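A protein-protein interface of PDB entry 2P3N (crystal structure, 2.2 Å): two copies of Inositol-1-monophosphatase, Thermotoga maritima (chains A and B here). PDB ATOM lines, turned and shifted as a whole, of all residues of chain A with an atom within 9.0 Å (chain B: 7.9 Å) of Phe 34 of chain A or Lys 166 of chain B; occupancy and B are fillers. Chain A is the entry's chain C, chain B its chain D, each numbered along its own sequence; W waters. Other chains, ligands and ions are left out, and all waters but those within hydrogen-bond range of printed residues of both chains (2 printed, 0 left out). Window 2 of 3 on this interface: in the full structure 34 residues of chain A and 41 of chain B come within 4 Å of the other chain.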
ATOM      1  N   VAL A  28       4.279  13.564  14.177  1.00  0.00           N
ATOM      2  CA  VAL A  28       4.100  14.335  12.947  1.00  0.00           C
ATOM      3  C   VAL A  28       3.148  15.502  13.212  1.00  0.00           C
ATOM      4  O   VAL A  28       2.011  15.292  13.644  1.00  0.00           O
ATOM      5  CB  VAL A  28       3.456  13.460  11.854  1.00  0.00           C
ATOM      6  CG1 VAL A  28       3.212  14.272  10.610  1.00  0.00           C
ATOM      7  CG2 VAL A  28       4.335  12.274  11.560  1.00  0.00           C
ATOM      8  N   GLU A  29       3.594  16.727  12.954  1.00  0.00           N
ATOM      9  CA  GLU A  29       2.725  17.880  13.178  1.00  0.00           C
ATOM     10  C   GLU A  29       2.194  18.430  11.861  1.00  0.00           C
ATOM     11  O   GLU A  29       2.889  18.390  10.846  1.00  0.00           O
ATOM     12  CB  GLU A  29       3.481  18.970  13.932  1.00  0.00           C
ATOM     13  CG  GLU A  29       4.068  18.487  15.239  1.00  0.00           C
ATOM     14  CD  GLU A  29       5.573  18.640  15.284  1.00  0.00           C
ATOM     15  OE1 GLU A  29       6.227  17.986  16.130  1.00  0.00           O
ATOM     16  OE2 GLU A  29       6.102  19.427  14.471  1.00  0.00           O
ATOM     17  N   LYS A  30       0.959  18.932  11.870  1.00  0.00           N
ATOM     18  CA  LYS A  30       0.366  19.490  10.661  1.00  0.00           C
ATOM     19  C   LYS A  30       0.728  20.961  10.599  1.00  0.00           C
ATOM     20  O   LYS A  30       0.522  21.686  11.564  1.00  0.00           O
ATOM     21  CB  LYS A  30      -1.158  19.327  10.677  1.00  0.00           C
ATOM     22  CG  LYS A  30      -1.644  17.889  10.855  1.00  0.00           C
ATOM     23  CD  LYS A  30      -3.160  17.765  10.703  1.00  0.00           C
ATOM     24  CE  LYS A  30      -3.663  16.387  11.147  1.00  0.00           C
ATOM     25  NZ  LYS A  30      -5.117  16.145  10.867  1.00  0.00           N
ATOM     26  N   LYS A  31       1.292  21.405   9.481  1.00  0.00           N
ATOM     27  CA  LYS A  31       1.661  22.810   9.349  1.00  0.00           C
ATOM     28  C   LYS A  31       0.422  23.589   8.881  1.00  0.00           C
ATOM     29  O   LYS A  31       0.059  24.610   9.468  1.00  0.00           O
ATOM     30  CB  LYS A  31       2.823  22.972   8.360  1.00  0.00           C
ATOM     31  CG  LYS A  31       3.877  23.980   8.829  1.00  0.00           C
ATOM     32  CD  LYS A  31       4.883  24.371   7.741  1.00  0.00           C
ATOM     33  CE  LYS A  31       5.791  23.222   7.353  1.00  0.00           C
ATOM     34  NZ  LYS A  31       6.900  23.664   6.452  1.00  0.00           N
ATOM     35  N   THR A  32      -0.230  23.087   7.834  1.00  0.00           N
ATOM     36  CA  THR A  32      -1.447  23.704   7.306  1.00  0.00           C
ATOM     37  C   THR A  32      -2.479  22.622   6.953  1.00  0.00           C
ATOM     38  O   THR A  32      -3.534  22.906   6.391  1.00  0.00           O
ATOM     39  CB  THR A  32      -1.166  24.532   6.034  1.00  0.00           C
ATOM     40  OG1 THR A  32      -0.950  23.650   4.926  1.00  0.00           O
ATOM     41  CG2 THR A  32       0.056  25.422   6.233  1.00  0.00           C
ATOM     42  N   GLY A  33      -2.159  21.379   7.287  1.00  0.00           N
ATOM     43  CA  GLY A  33      -3.047  20.274   6.993  1.00  0.00           C
ATOM     44  C   GLY A  33      -2.283  18.963   7.017  1.00  0.00           C
ATOM     45  O   GLY A  33      -1.062  18.948   7.225  1.00  0.00           O
ATOM     46  N   PHE A  34      -2.995  17.859   6.808  1.00  0.00           N
ATOM     47  CA  PHE A  34      -2.365  16.552   6.814  1.00  0.00           C
ATOM     48  C   PHE A  34      -1.472  16.342   5.592  1.00  0.00           C
ATOM     49  O   PHE A  34      -0.667  15.410   5.561  1.00  0.00           O
ATOM     50  CB  PHE A  34      -3.427  15.451   6.889  1.00  0.00           C
ATOM     51  CG  PHE A  34      -4.477  15.542   5.823  1.00  0.00           C
ATOM     52  CD1 PHE A  34      -5.429  16.551   5.847  1.00  0.00           C
ATOM     53  CD2 PHE A  34      -4.515  14.614   4.786  1.00  0.00           C
ATOM     54  CE1 PHE A  34      -6.402  16.632   4.857  1.00  0.00           C
ATOM     55  CE2 PHE A  34      -5.484  14.687   3.787  1.00  0.00           C
ATOM     56  CZ  PHE A  34      -6.429  15.697   3.823  1.00  0.00           C
ATOM     57  N   LYS A  35      -1.610  17.214   4.595  1.00  0.00           N
ATOM     58  CA  LYS A  35      -0.812  17.129   3.372  1.00  0.00           C
ATOM     59  C   LYS A  35       0.417  18.043   3.436  1.00  0.00           C
ATOM     60  O   LYS A  35       1.244  18.059   2.525  1.00  0.00           O
ATOM     61  CB  LYS A  35      -1.662  17.502   2.147  1.00  0.00           C
ATOM     62  CG  LYS A  35      -2.964  16.717   2.003  1.00  0.00           C
ATOM     63  CD  LYS A  35      -3.670  16.981   0.668  1.00  0.00           C
ATOM     64  CE  LYS A  35      -3.170  16.082  -0.472  1.00  0.00           C
ATOM     65  NZ  LYS A  35      -1.777  16.391  -0.900  1.00  0.00           N
ATOM     66  N   ASP A  36       0.516  18.824   4.503  1.00  0.00           N
ATOM     67  CA  ASP A  36       1.648  19.718   4.690  1.00  0.00           C
ATOM     68  C   ASP A  36       2.065  19.598   6.146  1.00  0.00           C
ATOM     69  O   ASP A  36       1.589  20.327   7.021  1.00  0.00           O
ATOM     70  CB  ASP A  36       1.273  21.156   4.372  1.00  0.00           C
ATOM     71  CG  ASP A  36       2.412  22.109   4.637  1.00  0.00           C
ATOM     72  OD1 ASP A  36       3.550  21.785   4.245  1.00  0.00           O
ATOM     73  OD2 ASP A  36       2.176  23.182   5.231  1.00  0.00           O
ATOM     74  N   ILE A  37       2.971  18.658   6.386  1.00  0.00           N
ATOM     75  CA  ILE A  37       3.444  18.349   7.722  1.00  0.00           C
ATOM     76  C   ILE A  37       4.887  18.747   7.965  1.00  0.00           C
ATOM     77  O   ILE A  37       5.605  19.180   7.056  1.00  0.00           O
ATOM     78  CB  ILE A  37       3.312  16.835   7.980  1.00  0.00           C
ATOM     79  CG1 ILE A  37       4.246  16.071   7.025  1.00  0.00           C
ATOM     80  CG2 ILE A  37       1.856  16.385   7.730  1.00  0.00           C
ATOM     81  CD1 ILE A  37       4.192  14.556   7.180  1.00  0.00           C
ATOM     82  N   VAL A  38       5.289  18.587   9.219  1.00  0.00           N
ATOM     83  CA  VAL A  38       6.631  18.883   9.676  1.00  0.00           C
ATOM     84  C   VAL A  38       6.879  18.062  10.948  1.00  0.00           C
ATOM     85  O   VAL A  38       5.931  17.646  11.635  1.00  0.00           O
ATOM     86  CB  VAL A  38       6.803  20.378   9.981  1.00  0.00           C
ATOM     87  CG1 VAL A  38       5.760  20.830  10.990  1.00  0.00           C
ATOM     88  CG2 VAL A  38       8.225  20.643  10.495  1.00  0.00           C
ATOM     89  N   THR A  84       9.110  15.531   3.546  1.00  0.00           N
ATOM     90  CA  THR A  84       8.904  15.094   4.927  1.00  0.00           C
ATOM     91  C   THR A  84       7.881  13.947   5.013  1.00  0.00           C
ATOM     92  O   THR A  84       7.982  13.077   5.891  1.00  0.00           O
ATOM     93  CB  THR A  84       8.433  16.277   5.835  1.00  0.00           C
ATOM     94  OG1 THR A  84       9.422  17.313   5.829  1.00  0.00           O
ATOM     95  CG2 THR A  84       8.244  15.819   7.276  1.00  0.00           C
ATOM     96  N   ILE A  85       6.901  13.942   4.110  1.00  0.00           N
ATOM     97  CA  ILE A  85       5.893  12.885   4.105  1.00  0.00           C
ATOM     98  C   ILE A  85       6.556  11.546   3.803  1.00  0.00           C
ATOM     99  O   ILE A  85       6.345  10.567   4.518  1.00  0.00           O
ATOM    100  CB  ILE A  85       4.773  13.199   3.080  1.00  0.00           C
ATOM    101  CG1 ILE A  85       3.930  14.364   3.626  1.00  0.00           C
ATOM    102  CG2 ILE A  85       3.923  11.959   2.805  1.00  0.00           C
ATOM    103  CD1 ILE A  85       2.655  14.632   2.874  1.00  0.00           C
ATOM    104  N   VAL A  88       8.717  10.364   6.638  1.00  0.00           N
ATOM    105  CA  VAL A  88       7.886   9.873   7.737  1.00  0.00           C
ATOM    106  C   VAL A  88       7.394   8.447   7.480  1.00  0.00           C
ATOM    107  O   VAL A  88       7.488   7.576   8.350  1.00  0.00           O
ATOM    108  CB  VAL A  88       6.651  10.796   7.934  1.00  0.00           C
ATOM    109  CG1 VAL A  88       5.625  10.129   8.850  1.00  0.00           C
ATOM    110  CG2 VAL A  88       7.098  12.138   8.513  1.00  0.00           C
ATOM    111  N   HIS A  89       6.878   8.220   6.276  1.00  0.00           N
ATOM    112  CA  HIS A  89       6.362   6.916   5.891  1.00  0.00           C
ATOM    113  C   HIS A  89       7.412   5.850   5.626  1.00  0.00           C
ATOM    114  O   HIS A  89       7.101   4.653   5.657  1.00  0.00           O
ATOM    115  CB  HIS A  89       5.440   7.068   4.678  1.00  0.00           C
ATOM    116  CG  HIS A  89       4.067   7.535   5.047  1.00  0.00           C
ATOM    117  ND1 HIS A  89       2.977   6.692   5.074  1.00  0.00           N
ATOM    118  CD2 HIS A  89       3.629   8.730   5.506  1.00  0.00           C
ATOM    119  CE1 HIS A  89       1.928   7.346   5.537  1.00  0.00           C
ATOM    120  NE2 HIS A  89       2.297   8.585   5.807  1.00  0.00           N
ATOM    121  N   TYR A 153      -0.431  18.078  -6.103  1.00  0.00           N
ATOM    122  CA  TYR A 153      -1.234  19.283  -5.953  1.00  0.00           C
ATOM    123  C   TYR A 153      -2.728  19.028  -6.076  1.00  0.00           C
ATOM    124  O   TYR A 153      -3.170  18.046  -6.670  1.00  0.00           O
ATOM    125  CB  TYR A 153      -0.807  20.309  -6.994  1.00  0.00           C
ATOM    126  CG  TYR A 153       0.693  20.408  -7.137  1.00  0.00           C
ATOM    127  CD1 TYR A 153       1.321  20.082  -8.339  1.00  0.00           C
ATOM    128  CD2 TYR A 153       1.491  20.799  -6.061  1.00  0.00           C
ATOM    129  CE1 TYR A 153       2.709  20.142  -8.468  1.00  0.00           C
ATOM    130  CE2 TYR A 153       2.878  20.862  -6.178  1.00  0.00           C
ATOM    131  CZ  TYR A 153       3.480  20.531  -7.384  1.00  0.00           C
ATOM    132  OH  TYR A 153       4.853  20.596  -7.502  1.00  0.00           O
ATOM    133  N   VAL A 154      -3.489  19.957  -5.515  1.00  0.00           N
ATOM    134  CA  VAL A 154      -4.939  19.905  -5.491  1.00  0.00           C
ATOM    135  C   VAL A 154      -5.627  19.536  -6.799  1.00  0.00           C
ATOM    136  O   VAL A 154      -6.078  18.403  -6.981  1.00  0.00           O
ATOM    137  CB  VAL A 154      -5.506  21.257  -5.003  1.00  0.00           C
ATOM    138  CG1 VAL A 154      -5.010  22.395  -5.904  1.00  0.00           C
ATOM    139  CG2 VAL A 154      -7.028  21.202  -4.963  1.00  0.00           C
ATOM    140  N   ASP A 155      -5.716  20.496  -7.708  1.00  0.00           N
ATOM    141  CA  ASP A 155      -6.387  20.278  -8.981  1.00  0.00           C
ATOM    142  C   ASP A 155      -5.391  19.839 -10.032  1.00  0.00           C
ATOM    143  O   ASP A 155      -5.609  18.875 -10.769  1.00  0.00           O
ATOM    144  CB  ASP A 155      -7.038  21.580  -9.436  1.00  0.00           C
ATOM    145  CG  ASP A 155      -7.571  22.393  -8.285  1.00  0.00           C
ATOM    146  OD1 ASP A 155      -8.527  21.934  -7.626  1.00  0.00           O
ATOM    147  OD2 ASP A 155      -7.022  23.488  -8.041  1.00  0.00           O
ATOM    148  N   SER B 142      -6.792   5.610   8.683  1.00  0.00           N
ATOM    149  CA  SER B 142      -7.610   6.549   7.918  1.00  0.00           C
ATOM    150  C   SER B 142      -6.829   7.086   6.724  1.00  0.00           C
ATOM    151  O   SER B 142      -5.652   7.415   6.854  1.00  0.00           O
ATOM    152  CB  SER B 142      -8.034   7.702   8.817  1.00  0.00           C
ATOM    153  OG  SER B 142      -6.925   8.178   9.559  1.00  0.00           O
ATOM    154  N   LEU B 143      -7.481   7.175   5.567  1.00  0.00           N
ATOM    155  CA  LEU B 143      -6.841   7.664   4.344  1.00  0.00           C
ATOM    156  C   LEU B 143      -6.013   8.942   4.511  1.00  0.00           C
ATOM    157  O   LEU B 143      -4.980   9.102   3.854  1.00  0.00           O
ATOM    158  CB  LEU B 143      -7.894   7.869   3.249  1.00  0.00           C
ATOM    159  CG  LEU B 143      -8.405   6.600   2.557  1.00  0.00           C
ATOM    160  CD1 LEU B 143      -9.531   6.927   1.594  1.00  0.00           C
ATOM    161  CD2 LEU B 143      -7.259   5.946   1.813  1.00  0.00           C
ATOM    162  N   GLU B 144      -6.462   9.846   5.381  1.00  0.00           N
ATOM    163  CA  GLU B 144      -5.745  11.099   5.644  1.00  0.00           C
ATOM    164  C   GLU B 144      -4.447  10.830   6.406  1.00  0.00           C
ATOM    165  O   GLU B 144      -3.660  11.741   6.674  1.00  0.00           O
ATOM    166  CB  GLU B 144      -6.616  12.066   6.462  1.00  0.00           C
ATOM    167  CG  GLU B 144      -7.753  12.727   5.684  1.00  0.00           C
ATOM    168  CD  GLU B 144      -8.879  11.766   5.313  1.00  0.00           C
ATOM    169  OE1 GLU B 144      -9.769  12.174   4.533  1.00  0.00           O
ATOM    170  OE2 GLU B 144      -8.882  10.615   5.805  1.00  0.00           O
ATOM    171  N   GLU B 145      -4.246   9.566   6.759  1.00  0.00           N
ATOM    172  CA  GLU B 145      -3.065   9.117   7.490  1.00  0.00           C
ATOM    173  C   GLU B 145      -2.204   8.265   6.569  1.00  0.00           C
ATOM    174  O   GLU B 145      -1.117   7.817   6.945  1.00  0.00           O
ATOM    175  CB  GLU B 145      -3.492   8.272   8.692  1.00  0.00           C
ATOM    176  CG  GLU B 145      -3.940   9.078   9.889  1.00  0.00           C
ATOM    177  CD  GLU B 145      -2.765   9.628  10.675  1.00  0.00           C
ATOM    178  OE1 GLU B 145      -2.960  10.595  11.442  1.00  0.00           O
ATOM    179  OE2 GLU B 145      -1.646   9.084  10.532  1.00  0.00           O
ATOM    180  N   CYS B 146      -2.694   8.070   5.353  1.00  0.00           N
ATOM    181  CA  CYS B 146      -2.023   7.221   4.391  1.00  0.00           C
ATOM    182  C   CYS B 146      -1.299   7.890   3.242  1.00  0.00           C
ATOM    183  O   CYS B 146      -1.378   9.104   3.051  1.00  0.00           O
ATOM    184  CB  CYS B 146      -3.037   6.240   3.800  1.00  0.00           C
ATOM    185  SG  CYS B 146      -3.781   5.139   5.007  1.00  0.00           S
ATOM    186  N   PHE B 160      -8.115   8.333 -10.514  1.00  0.00           N
ATOM    187  CA  PHE B 160      -7.711   7.880  -9.182  1.00  0.00           C
ATOM    188  C   PHE B 160      -7.020   8.998  -8.401  1.00  0.00           C
ATOM    189  O   PHE B 160      -7.264   9.169  -7.209  1.00  0.00           O
ATOM    190  CB  PHE B 160      -6.774   6.665  -9.328  1.00  0.00           C
ATOM    191  CG  PHE B 160      -6.454   5.963  -8.025  1.00  0.00           C
ATOM    192  CD1 PHE B 160      -5.414   6.408  -7.209  1.00  0.00           C
ATOM    193  CD2 PHE B 160      -7.193   4.851  -7.621  1.00  0.00           C
ATOM    194  CE1 PHE B 160      -5.114   5.750  -6.009  1.00  0.00           C
ATOM    195  CE2 PHE B 160      -6.901   4.189  -6.425  1.00  0.00           C
ATOM    196  CZ  PHE B 160      -5.860   4.639  -5.620  1.00  0.00           C
ATOM    197  N   ILE B 161      -6.162   9.755  -9.085  1.00  0.00           N
ATOM    198  CA  ILE B 161      -5.435  10.866  -8.475  1.00  0.00           C
ATOM    199  C   ILE B 161      -6.449  11.882  -8.000  1.00  0.00           C
ATOM    200  O   ILE B 161      -6.351  12.401  -6.897  1.00  0.00           O
ATOM    201  CB  ILE B 161      -4.525  11.606  -9.491  1.00  0.00           C
ATOM    202  CG1 ILE B 161      -3.540  10.636 -10.158  1.00  0.00           C
ATOM    203  CG2 ILE B 161      -3.796  12.748  -8.790  1.00  0.00           C
ATOM    204  CD1 ILE B 161      -2.517  10.028  -9.230  1.00  0.00           C
ATOM    205  N   GLU B 162      -7.416  12.166  -8.867  1.00  0.00           N
ATOM    206  CA  GLU B 162      -8.472  13.137  -8.591  1.00  0.00           C
ATOM    207  C   GLU B 162      -9.358  12.765  -7.412  1.00  0.00           C
ATOM    208  O   GLU B 162      -9.515  13.548  -6.478  1.00  0.00           O
ATOM    209  CB  GLU B 162      -9.345  13.328  -9.835  1.00  0.00           C
ATOM    210  CG  GLU B 162      -8.910  14.470 -10.733  1.00  0.00           C
ATOM    211  CD  GLU B 162      -9.789  14.610 -11.959  1.00  0.00           C
ATOM    212  OE1 GLU B 162     -11.029  14.543 -11.817  1.00  0.00           O
ATOM    213  OE2 GLU B 162      -9.236  14.798 -13.061  1.00  0.00           O
ATOM    214  N   ARG B 163      -9.936  11.570  -7.456  1.00  0.00           N
ATOM    215  CA  ARG B 163     -10.815  11.109  -6.390  1.00  0.00           C
ATOM    216  C   ARG B 163     -10.078  10.544  -5.182  1.00  0.00           C
ATOM    217  O   ARG B 163     -10.692   9.899  -4.334  1.00  0.00           O
ATOM    218  CB  ARG B 163     -11.769  10.044  -6.933  1.00  0.00           C
ATOM    219  CG  ARG B 163     -12.749  10.565  -7.958  1.00  0.00           C
ATOM    220  CD  ARG B 163     -13.602   9.443  -8.497  1.00  0.00           C
ATOM    221  NE  ARG B 163     -15.022   9.761  -8.397  1.00  0.00           N
ATOM    222  CZ  ARG B 163     -15.995   8.999  -8.891  1.00  0.00           C
ATOM    223  NH1 ARG B 163     -17.266   9.365  -8.752  1.00  0.00           N
ATOM    224  NH2 ARG B 163     -15.697   7.874  -9.533  1.00  0.00           N
ATOM    225  N   MET B 164      -8.775  10.792  -5.082  1.00  0.00           N
ATOM    226  CA  MET B 164      -8.011  10.252  -3.969  1.00  0.00           C
ATOM    227  C   MET B 164      -7.044  11.255  -3.332  1.00  0.00           C
ATOM    228  O   MET B 164      -6.607  11.060  -2.202  1.00  0.00           O
ATOM    229  CB  MET B 164      -7.249   9.016  -4.456  1.00  0.00           C
ATOM    230  CG  MET B 164      -6.773   8.069  -3.375  1.00  0.00           C
ATOM    231  SD  MET B 164      -8.094   7.133  -2.580  1.00  0.00           S
ATOM    232  CE  MET B 164      -8.128   5.670  -3.572  1.00  0.00           C
ATOM    233  N   GLU B 165      -6.729  12.339  -4.033  1.00  0.00           N
ATOM    234  CA  GLU B 165      -5.776  13.306  -3.494  1.00  0.00           C
ATOM    235  C   GLU B 165      -6.258  14.198  -2.366  1.00  0.00           C
ATOM    236  O   GLU B 165      -5.458  14.638  -1.537  1.00  0.00           O
ATOM    237  CB  GLU B 165      -5.186  14.169  -4.611  1.00  0.00           C
ATOM    238  CG  GLU B 165      -3.744  13.787  -4.951  1.00  0.00           C
ATOM    239  CD  GLU B 165      -2.810  13.868  -3.744  1.00  0.00           C
ATOM    240  OE1 GLU B 165      -2.521  14.992  -3.279  1.00  0.00           O
ATOM    241  OE2 GLU B 165      -2.371  12.805  -3.255  1.00  0.00           O
ATOM    242  N   LYS B 166      -7.550  14.480  -2.327  1.00  0.00           N
ATOM    243  CA  LYS B 166      -8.083  15.304  -1.248  1.00  0.00           C
ATOM    244  C   LYS B 166      -8.355  14.395  -0.047  1.00  0.00           C
ATOM    245  O   LYS B 166      -8.492  14.861   1.084  1.00  0.00           O
ATOM    246  CB  LYS B 166      -9.372  15.997  -1.701  1.00  0.00           C
ATOM    247  CG  LYS B 166     -10.345  15.078  -2.445  1.00  0.00           C
ATOM    248  CD  LYS B 166     -11.615  15.808  -2.896  1.00  0.00           C
ATOM    249  CE  LYS B 166     -12.462  16.268  -1.711  1.00  0.00           C
ATOM    250  NZ  LYS B 166     -12.930  15.120  -0.883  1.00  0.00           N
ATOM    251  N   ARG B 167      -8.407  13.091  -0.316  1.00  0.00           N
ATOM    252  CA  ARG B 167      -8.669  12.061   0.692  1.00  0.00           C
ATOM    253  C   ARG B 167      -7.420  11.541   1.416  1.00  0.00           C
ATOM    254  O   ARG B 167      -7.529  10.918   2.477  1.00  0.00           O
ATOM    255  CB  ARG B 167      -9.381  10.868   0.032  1.00  0.00           C
ATOM    256  CG  ARG B 167     -10.894  11.025  -0.154  1.00  0.00           C
ATOM    257  CD  ARG B 167     -11.657  10.621   1.130  1.00  0.00           C
ATOM    258  NE  ARG B 167     -12.125   9.230   1.113  1.00  0.00           N
ATOM    259  CZ  ARG B 167     -12.407   8.512   2.202  1.00  0.00           C
ATOM    260  NH1 ARG B 167     -12.260   9.049   3.412  1.00  0.00           N
ATOM    261  NH2 ARG B 167     -12.845   7.257   2.086  1.00  0.00           N
ATOM    262  N   THR B 168      -6.238  11.805   0.860  1.00  0.00           N
ATOM    263  CA  THR B 168      -5.004  11.297   1.449  1.00  0.00           C
ATOM    264  C   THR B 168      -3.812  12.269   1.353  1.00  0.00           C
ATOM    265  O   THR B 168      -3.854  13.234   0.591  1.00  0.00           O
ATOM    266  CB  THR B 168      -4.656   9.966   0.753  1.00  0.00           C
ATOM    267  OG1 THR B 168      -3.643   9.275   1.490  1.00  0.00           O
ATOM    268  CG2 THR B 168      -4.182  10.229  -0.669  1.00  0.00           C
ATOM    269  N   ARG B 169      -2.759  12.015   2.132  1.00  0.00           N
ATOM    270  CA  ARG B 169      -1.553  12.853   2.119  1.00  0.00           C
ATOM    271  C   ARG B 169      -0.981  12.999   0.716  1.00  0.00           C
ATOM    272  O   ARG B 169      -0.764  14.111   0.244  1.00  0.00           O
ATOM    273  CB  ARG B 169      -0.463  12.256   3.002  1.00  0.00           C
ATOM    274  CG  ARG B 169      -0.572  12.574   4.466  1.00  0.00           C
ATOM    275  CD  ARG B 169       0.153  11.528   5.315  1.00  0.00           C
ATOM    276  NE  ARG B 169       0.248  11.950   6.710  1.00  0.00           N
ATOM    277  CZ  ARG B 169       0.409  11.132   7.748  1.00  0.00           C
ATOM    278  NH1 ARG B 169       0.490   9.816   7.577  1.00  0.00           N
ATOM    279  NH2 ARG B 169       0.502  11.637   8.968  1.00  0.00           N
ATOM    280  N   ARG B 170      -0.725  11.870   0.058  1.00  0.00           N
ATOM    281  CA  ARG B 170      -0.174  11.857  -1.295  1.00  0.00           C
ATOM    282  C   ARG B 170      -0.368  10.516  -1.973  1.00  0.00           C
ATOM    283  O   ARG B 170      -0.502   9.499  -1.305  1.00  0.00           O
ATOM    284  CB  ARG B 170       1.322  12.192  -1.258  1.00  0.00           C
ATOM    285  CG  ARG B 170       1.595  13.685  -1.302  1.00  0.00           C
ATOM    286  CD  ARG B 170       2.949  14.029  -0.733  1.00  0.00           C
ATOM    287  NE  ARG B 170       3.218  15.471  -0.677  1.00  0.00           N
ATOM    288  CZ  ARG B 170       2.360  16.395  -0.253  1.00  0.00           C
ATOM    289  NH1 ARG B 170       1.147  16.062   0.147  1.00  0.00           N
ATOM    290  NH2 ARG B 170       2.739  17.658  -0.186  1.00  0.00           N
ATOM    291  N   ILE B 171      -0.416  10.522  -3.302  1.00  0.00           N
ATOM    292  CA  ILE B 171      -0.534   9.291  -4.080  1.00  0.00           C
ATOM    293  C   ILE B 171       0.760   9.259  -4.891  1.00  0.00           C
ATOM    294  O   ILE B 171       1.114  10.241  -5.546  1.00  0.00           O
ATOM    295  CB  ILE B 171      -1.746   9.309  -5.045  1.00  0.00           C
ATOM    296  CG1 ILE B 171      -3.057   9.393  -4.257  1.00  0.00           C
ATOM    297  CG2 ILE B 171      -1.734   8.047  -5.913  1.00  0.00           C
ATOM    298  CD1 ILE B 171      -3.419   8.136  -3.512  1.00  0.00           C
HETATM  299  O   HOH W   1       1.559   7.815   8.832  1.00  0.00           O
HETATM  300  O   HOH W   2       3.869  20.013   1.507  1.00  0.00           O
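The side-chain carboxylate of Glu 165 of chain B is in salt-bridge range of the side-chain amino group of Lys 35 of chain A, at 2.9 Å.
NZ of Lys 35 of chain A is in hydrogen-bond range of O of Arg 169 of chain B (2.7 Å).
O of Lys 35 of chain A lies within hydrogen-bond range of NH1 of Arg 170 of chain B (3.1 Å).
NE2 of His 89 of chain A is in hydrogen-bond range of NH1 of Arg 169 of chain B (2.8 Å).
The side-chain sulfur (SG) of Cys 146 of chain B lies within hydrogen-bond range of the backbone carbonyl oxygen (O) of Ser 142 of chain B (3.5 Å).
The side-chain hydroxyl of Thr 168 of chain B lies within hydrogen-bond range of the backbone carbonyl oxygen of Leu 143 of chain B (2.7 Å).
The side-chain carboxylate of Glu 145 of chain B is in salt-bridge range of the guanidinium group of Arg 169 of chain B (3.7 Å).
The side-chain hydroxyl (OG1) of Thr 168 of chain B lies within hydrogen-bond range of the backbone carbonyl oxygen (O) of Cys 146 of chain B (2.8 Å).
O of Cys 146 of chain B lies close to N of Arg 169 of chain B (3.4 Å).
OE2 of Glu 165 of chain B is in hydrogen-bond range of N of Ile 171 of chain B (3.0 Å).
O of Glu 144 of chain B touches CD2 of Phe 34 of chain A (3.5 Å).
Phe 34 of chain A touches Lys 166 of chain B.
Phe 34 of chain A touches Thr 168 of chain B (CE2 to C, 3.8 Å).
CG of Arg 169 of chain B touches O of Phe 34 of chain A, 3.0 Å away.
Thr 168 of chain B touches Lys 35 of chain A (O to CE, 3.1 Å).
Ile 85 of chain A touches Arg 169 of chain B.
CD1 of Ile 85 of chain A touches NH1 of Arg 170 of chain B, at 3.4 Å.
Glu 145 of chain B touches His 89 of chain A (O to CE1, 3.4 Å).
His 89 of chain A touches Cys 146 of chain B.
Glu 29 of chain A touches none of the printed residues of chain B.
Phe 34 of chain A touches just these residues of chain B: Glu 144 (3.5 Å), Lys 166 (3.5 Å), Thr 168 (3.8 Å) and Arg 169 (3.0 Å).
Of the printed residues of chain B, Lys 35 of chain A touches Glu 165, Thr 168, Arg 169 and Arg 170.
Leu 143 of chain B touches none of the printed residues of chain A.
Of the printed residues of chain A, Glu 144 of chain B touches Phe 34 (3.5 Å).
Of the printed residues of chain A, Cys 146 of chain B touches His 89.
Lys 166 of chain B touches just one residue of chain A: Phe 34 (3.5 Å).
Of the printed residues of chain A, Arg 170 of chain B touches Lys 35 (3.1 Å) and Ile 85 (3.4 Å).
The nearest residue of chain A that does not touch Lys 166 of chain B is Lys 35 of chain A (5.0 Å).
Printed residues of chain B that touch a printed residue of chain A: Glu 144, Glu 145, Cys 146, Glu 165, Lys 166, Thr 168, Arg 169 and Arg 170.
Of the 18 printed residues of chain A, 4 touch a printed residue of chain B.
Along chain A the printed residues that touch a printed residue of chain B span positions 34 to 89.
Among the printed residues, 13 pairs touch across the chains.
Among the printed residues, Asp or Glu carboxylates within 4 Å of a Lys or Arg side-chain nitrogen of the other chain: Lys 35 of chain A with Glu 165 of chain B.
No position is printed for both chains.
Of the 13 pairs that touch across the chains among the printed residues, none has its exchanged pair printed and touching as well.
Water W1 lies within hydrogen-bond range of NH1 of Arg 169 of chain B (2.6 Å), NE2 of His 89 of chain A (3.2 Å) and O of Glu 145 of chain B (3.3 Å).
Water W2 lies within hydrogen-bond range of NH2 of Arg 170 of chain B, OD1 of Asp 36 of chain A and O of Lys 35 of chain A.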
